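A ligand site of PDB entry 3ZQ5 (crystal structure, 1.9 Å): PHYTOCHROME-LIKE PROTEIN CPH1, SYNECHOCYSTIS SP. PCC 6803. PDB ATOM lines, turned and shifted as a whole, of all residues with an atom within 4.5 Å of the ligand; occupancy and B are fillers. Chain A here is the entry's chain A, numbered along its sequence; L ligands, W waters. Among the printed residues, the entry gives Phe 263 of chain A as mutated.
The side-chain sulfur (SG) of Cys 259 is bonded to a carbon (C23) of the ligand (1.6 Å). O6 of the ligand is in salt-bridge range of NH1 of Arg 254 (2.6 Å). OG1 of Thr 274 is in hydrogen-bond range of O1 of the ligand (2.6 Å). A ring nitrogen (NE2) of His 290 lies within hydrogen-bond range of an oxygen (O3) of the ligand, 2.7 Å away. The backbone NH (N) of Tyr 257 is in hydrogen-bond range of an oxygen (O6) of the ligand, 2.8 Å away. O of Asp 207 lies within hydrogen-bond range of N4 of the ligand, at 2.9 Å. A nitrogen (N1) of the ligand lies within hydrogen-bond range of a ring nitrogen (ND1) of His 260 (3.3 Å).
NH1 of Arg 254 lies within hydrogen-bond range of O of Ile 20 (3.3 Å). O of Arg 254 lies within hydrogen-bond range of NH2 of Arg 222 (2.8 Å). The backbone NH of Thr 274 lies within hydrogen-bond range of the backbone carbonyl oxygen of Arg 222, at 2.7 Å. The backbone NH (N) of Met 174 lies within hydrogen-bond range of the backbone carbonyl oxygen (O) of Ala 288, 2.8 Å away. O of Ser 272 lies within hydrogen-bond range of N of Ile 224 (2.9 Å). The backbone carbonyl oxygen (O) of Tyr 176 sits at hydrogen-bond distance from the backbone NH (N) of Leu 286 (2.8 Å).
Residues that only touch the ligand: Ser 206 (3.3 Å), Met 174 (3.3 Å), Ala 256 (3.4 Å), Pro 209 (3.5 Å), Tyr 203 (3.5 Å), Phe 216 (3.5 Å), Ile 208 (3.6 Å), Tyr 458 (3.6 Å), Leu 15 (3.6 Å), Leu 469 (3.6 Å), Val 186 (3.7 Å), Ala 212 (3.7 Å), Phe 263 (3.7 Å), Ile 20 (3.8 Å), Arg 222 (3.8 Å), Pro 471 (3.9 Å), Ile 224 (3.9 Å), Leu 18 (3.9 Å), Tyr 176 (3.9 Å) and Ala 457 (3.97 Å). Hydrophobic or aromatic side chains within 4 Å of the ligand: Leu 15, Leu 18, Ile 20, Met 174, Tyr 176, Val 186, Tyr 203, Ile 208, Pro 209, Ala 212, Phe 216, Ile 224, Ala 256, Tyr 257, His 260, Phe 263, His 290, Tyr 458, Leu 469 and Pro 471. Of the 32 residues printed, 27 come within 4 Å of the ligand.
Water W3 bridges O2 of the ligand (2.6 Å) and NE of Arg 222 (2.9 Å). Water W2 lies within hydrogen-bond range of an oxygen (O1) of the ligand, a ring nitrogen (NE2) of His 260 and the side-chain hydroxyl (OG) of Ser 272. Water W6 lies within hydrogen-bond range of the side-chain hydroxyl (OG) of Ser 272 (2.7 Å), an oxygen (O2) of the ligand (2.7 Å), the backbone carbonyl oxygen (O) of Arg 222 (3.1 Å) and the side-chain hydroxyl (OG1) of Thr 274 (3.3 Å). Water W4 lies within hydrogen-bond range of a ring nitrogen (ND1) of His 260, a nitrogen (N1) of the ligand and the backbone carbonyl oxygen (O) of Asp 207. Water W5 lies within hydrogen-bond range of a ring nitrogen (NE2) of His 290 (2.9 Å) and a nitrogen (N2) of the ligand (3.0 Å). Water W1 lies within hydrogen-bond range of OG of Ser 206, OD1 of Asp 207 and O of Ala 457.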
ATOM      1  N   LEU A  15       1.111 -33.398   3.230  1.00  0.00           N
ATOM      2  CA  LEU A  15       2.257 -32.712   3.834  1.00  0.00           C
ATOM      3  C   LEU A  15       3.263 -33.688   4.461  1.00  0.00           C
ATOM      4  O   LEU A  15       4.464 -33.500   4.323  1.00  0.00           O
ATOM      5  CB  LEU A  15       1.789 -31.693   4.884  1.00  0.00           C
ATOM      6  CG  LEU A  15       2.819 -30.698   5.435  1.00  0.00           C
ATOM      7  CD1 LEU A  15       3.297 -29.736   4.359  1.00  0.00           C
ATOM      8  CD2 LEU A  15       2.240 -29.928   6.614  1.00  0.00           C
ATOM      9  N   LEU A  18       5.168 -35.783   1.532  1.00  0.00           N
ATOM     10  CA  LEU A  18       5.804 -35.003   0.461  1.00  0.00           C
ATOM     11  C   LEU A  18       7.212 -35.526   0.124  1.00  0.00           C
ATOM     12  O   LEU A  18       8.081 -35.594   1.001  1.00  0.00           O
ATOM     13  CB  LEU A  18       5.897 -33.539   0.905  1.00  0.00           C
ATOM     14  CG  LEU A  18       5.628 -32.370  -0.037  1.00  0.00           C
ATOM     15  CD1 LEU A  18       4.376 -32.571  -0.884  1.00  0.00           C
ATOM     16  CD2 LEU A  18       5.509 -31.111   0.811  1.00  0.00           C
ATOM     17  N   ILE A  20      10.154 -34.626  -0.889  1.00  0.00           N
ATOM     18  CA  ILE A  20      11.058 -33.493  -1.116  1.00  0.00           C
ATOM     19  C   ILE A  20      12.448 -33.948  -1.590  1.00  0.00           C
ATOM     20  O   ILE A  20      13.153 -33.178  -2.235  1.00  0.00           O
ATOM     21  CB  ILE A  20      11.207 -32.580   0.132  1.00  0.00           C
ATOM     22  CG1 ILE A  20      11.749 -33.378   1.345  1.00  0.00           C
ATOM     23  CG2 ILE A  20       9.873 -31.902   0.464  1.00  0.00           C
ATOM     24  CD1 ILE A  20      12.274 -32.478   2.502  1.00  0.00           C
ATOM     25  N   MET A 174      19.289 -18.978  15.679  1.00  0.00           N
ATOM     26  CA  MET A 174      18.385 -19.551  16.673  1.00  0.00           C
ATOM     27  C   MET A 174      18.707 -21.015  17.003  1.00  0.00           C
ATOM     28  O   MET A 174      19.302 -21.736  16.183  1.00  0.00           O
ATOM     29  CB  MET A 174      16.961 -19.468  16.131  1.00  0.00           C
ATOM     30  CG  MET A 174      16.471 -18.019  16.023  1.00  0.00           C
ATOM     31  SD  MET A 174      14.893 -17.913  15.199  1.00  0.00           S
ATOM     32  CE  MET A 174      15.333 -18.575  13.574  1.00  0.00           C
ATOM     33  N   TYR A 176      16.403 -24.250  17.858  1.00  0.00           N
ATOM     34  CA  TYR A 176      15.040 -24.666  17.687  1.00  0.00           C
ATOM     35  C   TYR A 176      14.920 -26.101  18.173  1.00  0.00           C
ATOM     36  O   TYR A 176      15.518 -26.983  17.598  1.00  0.00           O
ATOM     37  CB  TYR A 176      14.717 -24.587  16.210  1.00  0.00           C
ATOM     38  CG  TYR A 176      13.283 -24.746  15.812  1.00  0.00           C
ATOM     39  CD1 TYR A 176      12.749 -26.012  15.542  1.00  0.00           C
ATOM     40  CD2 TYR A 176      12.475 -23.633  15.608  1.00  0.00           C
ATOM     41  CE1 TYR A 176      11.446 -26.170  15.142  1.00  0.00           C
ATOM     42  CE2 TYR A 176      11.149 -23.787  15.189  1.00  0.00           C
ATOM     43  CZ  TYR A 176      10.645 -25.049  14.958  1.00  0.00           C
ATOM     44  OH  TYR A 176       9.349 -25.213  14.542  1.00  0.00           O
ATOM     45  N   VAL A 186      11.684 -21.974  19.969  1.00  0.00           N
ATOM     46  CA  VAL A 186      12.928 -21.221  19.864  1.00  0.00           C
ATOM     47  C   VAL A 186      13.450 -20.979  21.282  1.00  0.00           C
ATOM     48  O   VAL A 186      12.917 -20.166  22.010  1.00  0.00           O
ATOM     49  CB  VAL A 186      12.738 -19.898  19.110  1.00  0.00           C
ATOM     50  CG1 VAL A 186      14.076 -19.145  18.999  1.00  0.00           C
ATOM     51  CG2 VAL A 186      12.122 -20.161  17.720  1.00  0.00           C
ATOM     52  N   TYR A 203       6.060 -23.206  17.513  1.00  0.00           N
ATOM     53  CA  TYR A 203       5.557 -23.404  16.133  1.00  0.00           C
ATOM     54  C   TYR A 203       4.929 -24.793  15.947  1.00  0.00           C
ATOM     55  O   TYR A 203       5.404 -25.759  16.557  1.00  0.00           O
ATOM     56  CB  TYR A 203       6.718 -23.234  15.151  1.00  0.00           C
ATOM     57  CG  TYR A 203       7.230 -21.824  15.094  1.00  0.00           C
ATOM     58  CD1 TYR A 203       8.225 -21.393  15.947  1.00  0.00           C
ATOM     59  CD2 TYR A 203       6.687 -20.905  14.196  1.00  0.00           C
ATOM     60  CE1 TYR A 203       8.692 -20.095  15.910  1.00  0.00           C
ATOM     61  CE2 TYR A 203       7.145 -19.601  14.160  1.00  0.00           C
ATOM     62  CZ  TYR A 203       8.142 -19.206  15.014  1.00  0.00           C
ATOM     63  OH  TYR A 203       8.601 -17.919  14.979  1.00  0.00           O
ATOM     64  N   SER A 206       3.749 -28.965  11.704  1.00  0.00           N
ATOM     65  CA  SER A 206       3.648 -28.895  10.249  1.00  0.00           C
ATOM     66  C   SER A 206       4.594 -27.875   9.587  1.00  0.00           C
ATOM     67  O   SER A 206       4.792 -27.932   8.380  1.00  0.00           O
ATOM     68  CB  SER A 206       2.204 -28.635   9.813  1.00  0.00           C
ATOM     69  OG  SER A 206       1.662 -27.508  10.467  1.00  0.00           O
ATOM     70  N   ASP A 207       5.167 -26.957  10.366  1.00  0.00           N
ATOM     71  CA  ASP A 207       6.140 -25.990   9.854  1.00  0.00           C
ATOM     72  C   ASP A 207       7.417 -26.679   9.365  1.00  0.00           C
ATOM     73  O   ASP A 207       8.003 -26.270   8.372  1.00  0.00           O
ATOM     74  CB  ASP A 207       6.513 -24.942  10.908  1.00  0.00           C
ATOM     75  CG  ASP A 207       5.480 -23.814  11.003  1.00  0.00           C
ATOM     76  OD1 ASP A 207       4.297 -24.014  10.654  1.00  0.00           O
ATOM     77  OD2 ASP A 207       5.867 -22.705  11.416  1.00  0.00           O
ATOM     78  N   ILE A 208       7.840 -27.706  10.093  1.00  0.00           N
ATOM     79  CA  ILE A 208       8.902 -28.590   9.658  1.00  0.00           C
ATOM     80  C   ILE A 208       8.372 -30.012   9.610  1.00  0.00           C
ATOM     81  O   ILE A 208       8.517 -30.746  10.585  1.00  0.00           O
ATOM     82  CB  ILE A 208      10.111 -28.508  10.596  1.00  0.00           C
ATOM     83  CG1 ILE A 208      10.381 -27.055  10.968  1.00  0.00           C
ATOM     84  CG2 ILE A 208      11.331 -29.168   9.942  1.00  0.00           C
ATOM     85  CD1 ILE A 208      11.679 -26.826  11.736  1.00  0.00           C
ATOM     86  N   PRO A 209       7.745 -30.406   8.494  1.00  0.00           N
ATOM     87  CA  PRO A 209       6.995 -31.663   8.522  1.00  0.00           C
ATOM     88  C   PRO A 209       7.884 -32.912   8.481  1.00  0.00           C
ATOM     89  O   PRO A 209       9.108 -32.817   8.324  1.00  0.00           O
ATOM     90  CB  PRO A 209       6.103 -31.576   7.268  1.00  0.00           C
ATOM     91  CG  PRO A 209       6.771 -30.601   6.360  1.00  0.00           C
ATOM     92  CD  PRO A 209       7.549 -29.655   7.232  1.00  0.00           C
ATOM     93  N   ALA A 212      10.834 -33.316   6.102  1.00  0.00           N
ATOM     94  CA  ALA A 212      11.929 -32.383   6.376  1.00  0.00           C
ATOM     95  C   ALA A 212      12.741 -32.866   7.564  1.00  0.00           C
ATOM     96  O   ALA A 212      13.968 -32.857   7.526  1.00  0.00           O
ATOM     97  CB  ALA A 212      11.391 -30.987   6.635  1.00  0.00           C
ATOM     98  N   PHE A 216      16.826 -34.411   7.734  1.00  0.00           N
ATOM     99  CA  PHE A 216      17.897 -33.962   8.640  1.00  0.00           C
ATOM    100  C   PHE A 216      18.610 -35.050   9.441  1.00  0.00           C
ATOM    101  O   PHE A 216      19.715 -34.809   9.969  1.00  0.00           O
ATOM    102  CB  PHE A 216      17.373 -32.888   9.594  1.00  0.00           C
ATOM    103  CG  PHE A 216      17.417 -31.520   9.007  1.00  0.00           C
ATOM    104  CD1 PHE A 216      18.637 -30.924   8.693  1.00  0.00           C
ATOM    105  CD2 PHE A 216      16.256 -30.823   8.752  1.00  0.00           C
ATOM    106  CE1 PHE A 216      18.688 -29.646   8.160  1.00  0.00           C
ATOM    107  CE2 PHE A 216      16.292 -29.565   8.187  1.00  0.00           C
ATOM    108  CZ  PHE A 216      17.511 -28.973   7.894  1.00  0.00           C
ATOM    109  N   ARG A 222      21.601 -28.053   5.903  1.00  0.00           N
ATOM    110  CA  ARG A 222      20.968 -27.442   4.742  1.00  0.00           C
ATOM    111  C   ARG A 222      21.363 -25.984   4.626  1.00  0.00           C
ATOM    112  O   ARG A 222      21.334 -25.257   5.615  1.00  0.00           O
ATOM    113  CB  ARG A 222      19.459 -27.617   4.805  1.00  0.00           C
ATOM    114  CG  ARG A 222      19.012 -29.011   4.424  1.00  0.00           C
ATOM    115  CD  ARG A 222      19.190 -29.277   2.895  1.00  0.00           C
ATOM    116  NE  ARG A 222      18.291 -28.394   2.138  1.00  0.00           N
ATOM    117  CZ  ARG A 222      18.395 -28.102   0.850  1.00  0.00           C
ATOM    118  NH1 ARG A 222      19.345 -28.627   0.080  1.00  0.00           N
ATOM    119  NH2 ARG A 222      17.495 -27.272   0.311  1.00  0.00           N
ATOM    120  N   ILE A 224      20.871 -22.428   2.051  1.00  0.00           N
ATOM    121  CA  ILE A 224      20.216 -21.694   0.957  1.00  0.00           C
ATOM    122  C   ILE A 224      20.827 -20.292   0.866  1.00  0.00           C
ATOM    123  O   ILE A 224      20.373 -19.389   1.571  1.00  0.00           O
ATOM    124  CB  ILE A 224      18.689 -21.583   1.176  1.00  0.00           C
ATOM    125  CG1 ILE A 224      18.095 -22.968   1.464  1.00  0.00           C
ATOM    126  CG2 ILE A 224      17.998 -20.957  -0.071  1.00  0.00           C
ATOM    127  CD1 ILE A 224      16.587 -22.937   1.800  1.00  0.00           C
ATOM    128  N   ARG A 254      20.179 -29.161  -3.853  1.00  0.00           N
ATOM    129  CA  ARG A 254      18.736 -29.361  -3.926  1.00  0.00           C
ATOM    130  C   ARG A 254      18.021 -28.086  -3.459  1.00  0.00           C
ATOM    131  O   ARG A 254      18.305 -27.574  -2.369  1.00  0.00           O
ATOM    132  CB  ARG A 254      18.271 -30.548  -3.081  1.00  0.00           C
ATOM    133  CG  ARG A 254      16.799 -30.952  -3.360  1.00  0.00           C
ATOM    134  CD  ARG A 254      16.350 -32.070  -2.435  1.00  0.00           C
ATOM    135  NE  ARG A 254      16.564 -31.673  -1.044  1.00  0.00           N
ATOM    136  CZ  ARG A 254      15.704 -30.965  -0.303  1.00  0.00           C
ATOM    137  NH1 ARG A 254      14.524 -30.582  -0.787  1.00  0.00           N
ATOM    138  NH2 ARG A 254      16.036 -30.640   0.927  1.00  0.00           N
ATOM    139  N   SER A 255      17.153 -27.571  -4.313  1.00  0.00           N
ATOM    140  CA  SER A 255      16.326 -26.414  -3.996  1.00  0.00           C
ATOM    141  C   SER A 255      15.208 -26.846  -3.068  1.00  0.00           C
ATOM    142  O   SER A 255      14.585 -27.888  -3.276  1.00  0.00           O
ATOM    143  CB  SER A 255      15.735 -25.814  -5.276  1.00  0.00           C
ATOM    144  OG  SER A 255      15.048 -24.598  -4.995  1.00  0.00           O
ATOM    145  N   ALA A 256      14.935 -26.039  -2.059  1.00  0.00           N
ATOM    146  CA  ALA A 256      13.909 -26.353  -1.080  1.00  0.00           C
ATOM    147  C   ALA A 256      12.540 -26.341  -1.703  1.00  0.00           C
ATOM    148  O   ALA A 256      12.279 -25.654  -2.703  1.00  0.00           O
ATOM    149  CB  ALA A 256      13.979 -25.393   0.147  1.00  0.00           C
ATOM    150  N   TYR A 257      11.638 -27.096  -1.106  1.00  0.00           N
ATOM    151  CA  TYR A 257      10.257 -27.145  -1.560  1.00  0.00           C
ATOM    152  C   TYR A 257       9.697 -25.728  -1.550  1.00  0.00           C
ATOM    153  O   TYR A 257      10.018 -24.923  -0.660  1.00  0.00           O
ATOM    154  CB  TYR A 257       9.457 -28.099  -0.671  1.00  0.00           C
ATOM    155  CG  TYR A 257       8.075 -28.387  -1.154  1.00  0.00           C
ATOM    156  CD1 TYR A 257       7.858 -29.248  -2.210  1.00  0.00           C
ATOM    157  CD2 TYR A 257       6.972 -27.798  -0.546  1.00  0.00           C
ATOM    158  CE1 TYR A 257       6.576 -29.512  -2.679  1.00  0.00           C
ATOM    159  CE2 TYR A 257       5.684 -28.056  -0.999  1.00  0.00           C
ATOM    160  CZ  TYR A 257       5.486 -28.922  -2.065  1.00  0.00           C
ATOM    161  OH  TYR A 257       4.226 -29.191  -2.529  1.00  0.00           O
ATOM    162  N   CYS A 259       7.050 -24.117  -0.888  1.00  0.00           N
ATOM    163  CA  CYS A 259       6.298 -23.574   0.234  1.00  0.00           C
ATOM    164  C   CYS A 259       7.222 -23.066   1.334  1.00  0.00           C
ATOM    165  O   CYS A 259       6.936 -22.063   2.005  1.00  0.00           O
ATOM    166  CB  CYS A 259       5.348 -24.624   0.798  1.00  0.00           C
ATOM    167  SG  CYS A 259       4.622 -24.204   2.417  1.00  0.00           S
ATOM    168  N   HIS A 260       8.346 -23.757   1.530  1.00  0.00           N
ATOM    169  CA  HIS A 260       9.348 -23.292   2.487  1.00  0.00           C
ATOM    170  C   HIS A 260      10.072 -22.031   2.004  1.00  0.00           C
ATOM    171  O   HIS A 260      10.310 -21.115   2.776  1.00  0.00           O
ATOM    172  CB  HIS A 260      10.394 -24.381   2.780  1.00  0.00           C
ATOM    173  CG  HIS A 260      11.450 -23.925   3.738  1.00  0.00           C
ATOM    174  ND1 HIS A 260      11.149 -23.420   4.982  1.00  0.00           N
ATOM    175  CD2 HIS A 260      12.787 -23.862   3.611  1.00  0.00           C
ATOM    176  CE1 HIS A 260      12.265 -23.082   5.596  1.00  0.00           C
ATOM    177  NE2 HIS A 260      13.279 -23.333   4.787  1.00  0.00           N
ATOM    178  N   PHE A 263       7.694 -19.275   2.577  1.00  0.00           N
ATOM    179  CA  PHE A 263       7.778 -18.976   4.006  1.00  0.00           C
ATOM    180  C   PHE A 263       8.955 -18.070   4.328  1.00  0.00           C
ATOM    181  O   PHE A 263       8.801 -17.070   5.032  1.00  0.00           O
ATOM    182  CB  PHE A 263       7.867 -20.278   4.814  1.00  0.00           C
ATOM    183  CG  PHE A 263       8.182 -20.068   6.275  1.00  0.00           C
ATOM    184  CD1 PHE A 263       7.197 -19.650   7.149  1.00  0.00           C
ATOM    185  CD2 PHE A 263       9.457 -20.302   6.759  1.00  0.00           C
ATOM    186  CE1 PHE A 263       7.487 -19.465   8.508  1.00  0.00           C
ATOM    187  CE2 PHE A 263       9.747 -20.116   8.118  1.00  0.00           C
ATOM    188  CZ  PHE A 263       8.765 -19.692   8.984  1.00  0.00           C
ATOM    189  N   SER A 272      19.701 -18.742   4.277  1.00  0.00           N
ATOM    190  CA  SER A 272      19.634 -19.528   5.496  1.00  0.00           C
ATOM    191  C   SER A 272      20.673 -20.635   5.584  1.00  0.00           C
ATOM    192  O   SER A 272      21.217 -21.109   4.563  1.00  0.00           O
ATOM    193  CB  SER A 272      18.232 -20.108   5.655  1.00  0.00           C
ATOM    194  OG  SER A 272      18.032 -21.191   4.766  1.00  0.00           O
ATOM    195  N   THR A 274      21.034 -24.245   8.151  1.00  0.00           N
ATOM    196  CA  THR A 274      20.333 -25.042   9.160  1.00  0.00           C
ATOM    197  C   THR A 274      21.150 -26.280   9.421  1.00  0.00           C
ATOM    198  O   THR A 274      21.518 -26.986   8.479  1.00  0.00           O
ATOM    199  CB  THR A 274      18.902 -25.391   8.681  1.00  0.00           C
ATOM    200  OG1 THR A 274      18.218 -24.188   8.291  1.00  0.00           O
ATOM    201  CG2 THR A 274      18.102 -26.092   9.761  1.00  0.00           C
ATOM    202  N   LEU A 286      17.452 -27.972  15.857  1.00  0.00           N
ATOM    203  CA  LEU A 286      18.155 -27.382  14.752  1.00  0.00           C
ATOM    204  C   LEU A 286      18.821 -26.104  15.219  1.00  0.00           C
ATOM    205  O   LEU A 286      18.261 -25.364  16.026  1.00  0.00           O
ATOM    206  CB  LEU A 286      17.201 -27.068  13.586  1.00  0.00           C
ATOM    207  CG  LEU A 286      16.313 -28.155  13.008  1.00  0.00           C
ATOM    208  CD1 LEU A 286      15.329 -27.561  12.029  1.00  0.00           C
ATOM    209  CD2 LEU A 286      17.129 -29.243  12.352  1.00  0.00           C
ATOM    210  N   ALA A 288      19.300 -22.830  13.520  1.00  0.00           N
ATOM    211  CA  ALA A 288      18.644 -22.203  12.375  1.00  0.00           C
ATOM    212  C   ALA A 288      19.162 -20.787  12.210  1.00  0.00           C
ATOM    213  O   ALA A 288      18.987 -19.975  13.091  1.00  0.00           O
ATOM    214  CB  ALA A 288      17.150 -22.224  12.577  1.00  0.00           C
ATOM    215  N   HIS A 290      19.388 -17.197   9.840  1.00  0.00           N
ATOM    216  CA  HIS A 290      18.791 -16.359   8.789  1.00  0.00           C
ATOM    217  C   HIS A 290      19.641 -15.119   8.541  1.00  0.00           C
ATOM    218  O   HIS A 290      20.122 -14.446   9.496  1.00  0.00           O
ATOM    219  CB  HIS A 290      17.426 -15.818   9.205  1.00  0.00           C
ATOM    220  CG  HIS A 290      16.358 -16.843   9.347  1.00  0.00           C
ATOM    221  ND1 HIS A 290      15.132 -16.552   9.917  1.00  0.00           N
ATOM    222  CD2 HIS A 290      16.301 -18.150   8.989  1.00  0.00           C
ATOM    223  CE1 HIS A 290      14.371 -17.633   9.901  1.00  0.00           C
ATOM    224  NE2 HIS A 290      15.062 -18.618   9.362  1.00  0.00           N
ATOM    225  N   ALA A 457      -2.623 -23.508  10.392  1.00  0.00           N
ATOM    226  CA  ALA A 457      -1.162 -23.592  10.436  1.00  0.00           C
ATOM    227  C   ALA A 457      -0.546 -23.508   9.044  1.00  0.00           C
ATOM    228  O   ALA A 457       0.661 -23.326   8.891  1.00  0.00           O
ATOM    229  CB  ALA A 457      -0.734 -24.887  11.129  1.00  0.00           C
ATOM    230  N   TYR A 458      -1.375 -23.671   8.018  1.00  0.00           N
ATOM    231  CA  TYR A 458      -0.943 -23.487   6.645  1.00  0.00           C
ATOM    232  C   TYR A 458      -2.183 -23.312   5.788  1.00  0.00           C
ATOM    233  O   TYR A 458      -3.302 -23.389   6.301  1.00  0.00           O
ATOM    234  CB  TYR A 458      -0.123 -24.687   6.167  1.00  0.00           C
ATOM    235  CG  TYR A 458      -0.842 -26.005   6.316  1.00  0.00           C
ATOM    236  CD1 TYR A 458      -0.809 -26.706   7.518  1.00  0.00           C
ATOM    237  CD2 TYR A 458      -1.557 -26.547   5.255  1.00  0.00           C
ATOM    238  CE1 TYR A 458      -1.483 -27.917   7.670  1.00  0.00           C
ATOM    239  CE2 TYR A 458      -2.234 -27.759   5.393  1.00  0.00           C
ATOM    240  CZ  TYR A 458      -2.197 -28.435   6.600  1.00  0.00           C
ATOM    241  OH  TYR A 458      -2.865 -29.631   6.714  1.00  0.00           O
ATOM    242  N   LEU A 469      -0.191 -26.758  -1.194  1.00  0.00           N
ATOM    243  CA  LEU A 469      -0.039 -26.268   0.164  1.00  0.00           C
ATOM    244  C   LEU A 469       0.857 -25.048   0.162  1.00  0.00           C
ATOM    245  O   LEU A 469       1.834 -24.992  -0.597  1.00  0.00           O
ATOM    246  CB  LEU A 469       0.541 -27.353   1.060  1.00  0.00           C
ATOM    247  CG  LEU A 469      -0.243 -28.668   1.125  1.00  0.00           C
ATOM    248  CD1 LEU A 469       0.544 -29.743   1.873  1.00  0.00           C
ATOM    249  CD2 LEU A 469      -1.607 -28.456   1.768  1.00  0.00           C
ATOM    250  N   HIS A 470       0.498 -24.070   0.993  1.00  0.00           N
ATOM    251  CA  HIS A 470       1.168 -22.767   1.058  1.00  0.00           C
ATOM    252  C   HIS A 470       1.409 -22.393   2.518  1.00  0.00           C
ATOM    253  O   HIS A 470       0.658 -22.824   3.413  1.00  0.00           O
ATOM    254  CB  HIS A 470       0.315 -21.678   0.411  1.00  0.00           C
ATOM    255  CG  HIS A 470      -0.187 -22.027  -0.961  1.00  0.00           C
ATOM    256  ND1 HIS A 470       0.576 -21.840  -2.099  1.00  0.00           N
ATOM    257  CD2 HIS A 470      -1.375 -22.543  -1.369  1.00  0.00           C
ATOM    258  CE1 HIS A 470      -0.125 -22.230  -3.149  1.00  0.00           C
ATOM    259  NE2 HIS A 470      -1.303 -22.663  -2.743  1.00  0.00           N
ATOM    260  N   PRO A 471       2.442 -21.575   2.779  1.00  0.00           N
ATOM    261  CA  PRO A 471       2.634 -21.116   4.155  1.00  0.00           C
ATOM    262  C   PRO A 471       1.519 -20.162   4.558  1.00  0.00           C
ATOM    263  O   PRO A 471       0.808 -19.622   3.689  1.00  0.00           O
ATOM    264  CB  PRO A 471       3.983 -20.394   4.117  1.00  0.00           C
ATOM    265  CG  PRO A 471       4.225 -20.054   2.708  1.00  0.00           C
ATOM    266  CD  PRO A 471       3.302 -20.852   1.825  1.00  0.00           C
HETATM  267  C1  LIG L   1      11.413 -26.972   6.087  1.00  0.00           C
HETATM  268  N1  LIG L   1      10.831 -25.211   7.737  1.00  0.00           N
HETATM  269  C2  LIG L   1      11.697 -26.049   7.174  1.00  0.00           C
HETATM  270  C3  LIG L   1      13.060 -25.967   7.721  1.00  0.00           C
HETATM  271  C4  LIG L   1      12.930 -24.958   8.771  1.00  0.00           C
HETATM  272  C5  LIG L   1      11.592 -24.541   8.662  1.00  0.00           C
HETATM  273  C6  LIG L   1      14.066 -24.500   9.668  1.00  0.00           C
HETATM  274  C7  LIG L   1      14.266 -26.799   7.336  1.00  0.00           C
HETATM  275  C8  LIG L   1      14.798 -26.582   5.919  1.00  0.00           C
HETATM  276  C9  LIG L   1      15.841 -25.517   5.885  1.00  0.00           C
HETATM  277  O1  LIG L   1      16.046 -24.844   6.933  1.00  0.00           O
HETATM  278  O2  LIG L   1      16.449 -25.342   4.810  1.00  0.00           O
HETATM  279  C10 LIG L   1      10.820 -23.787   9.646  1.00  0.00           C
HETATM  280  N2  LIG L   1      12.548 -22.077  10.136  1.00  0.00           N
HETATM  281  C11 LIG L   1      11.313 -22.593  10.362  1.00  0.00           C
HETATM  282  C12 LIG L   1      10.613 -21.870  11.324  1.00  0.00           C
HETATM  283  C13 LIG L   1      11.409 -20.830  11.745  1.00  0.00           C
HETATM  284  C14 LIG L   1      12.543 -21.010  10.966  1.00  0.00           C
HETATM  285  C15 LIG L   1       9.238 -22.172  11.791  1.00  0.00           C
HETATM  286  C16 LIG L   1      11.113 -19.723  12.753  1.00  0.00           C
HETATM  287  C17 LIG L   1      11.699 -20.078  14.091  1.00  0.00           C
HETATM  288  O3  LIG L   1      13.694 -20.121  11.114  1.00  0.00           O
HETATM  289  N3  LIG L   1       6.330 -25.134   5.843  1.00  0.00           N
HETATM  290  C18 LIG L   1       5.386 -24.305   6.002  1.00  0.00           C
HETATM  291  C19 LIG L   1       4.062 -24.869   5.600  1.00  0.00           C
HETATM  292  C20 LIG L   1       4.506 -25.977   4.644  1.00  0.00           C
HETATM  293  C21 LIG L   1       5.958 -26.102   5.013  1.00  0.00           C
HETATM  294  C22 LIG L   1       3.321 -25.404   6.806  1.00  0.00           C
HETATM  295  C23 LIG L   1       4.421 -25.618   3.169  1.00  0.00           C
HETATM  296  C24 LIG L   1       3.880 -26.779   2.358  1.00  0.00           C
HETATM  297  O4  LIG L   1       5.511 -23.053   6.448  1.00  0.00           O
HETATM  298  C25 LIG L   1       6.691 -27.122   4.529  1.00  0.00           C
HETATM  299  N4  LIG L   1       8.929 -26.794   5.641  1.00  0.00           N
HETATM  300  C26 LIG L   1       8.151 -27.391   4.684  1.00  0.00           C
HETATM  301  C27 LIG L   1       8.860 -28.269   3.730  1.00  0.00           C
HETATM  302  C28 LIG L   1      10.226 -28.239   4.280  1.00  0.00           C
HETATM  303  C29 LIG L   1      10.163 -27.243   5.358  1.00  0.00           C
HETATM  304  C30 LIG L   1       8.261 -29.063   2.583  1.00  0.00           C
HETATM  305  C31 LIG L   1      11.545 -28.672   3.771  1.00  0.00           C
HETATM  306  C32 LIG L   1      11.704 -28.569   2.458  1.00  0.00           C
HETATM  307  C33 LIG L   1      12.953 -28.872   1.722  1.00  0.00           C
HETATM  308  O5  LIG L   1      14.080 -28.955   2.259  1.00  0.00           O
HETATM  309  O6  LIG L   1      12.770 -29.097   0.502  1.00  0.00           O
HETATM  310  O   HOH W   1       2.396 -25.293   9.833  1.00  0.00           O
HETATM  311  O   HOH W   2      15.633 -22.439   5.958  1.00  0.00           O
HETATM  312  O   HOH W   3      15.917 -26.935   2.816  1.00  0.00           O
HETATM  313  O   HOH W   4       8.800 -23.679   6.330  1.00  0.00           O
HETATM  314  O   HOH W   5      14.953 -21.372   8.511  1.00  0.00           O
HETATM  315  O   HOH W   6      18.690 -23.780   5.034  1.00  0.00           O
HETATM  316  O   HOH W   7       3.483 -21.488   7.439  1.00  0.00           O
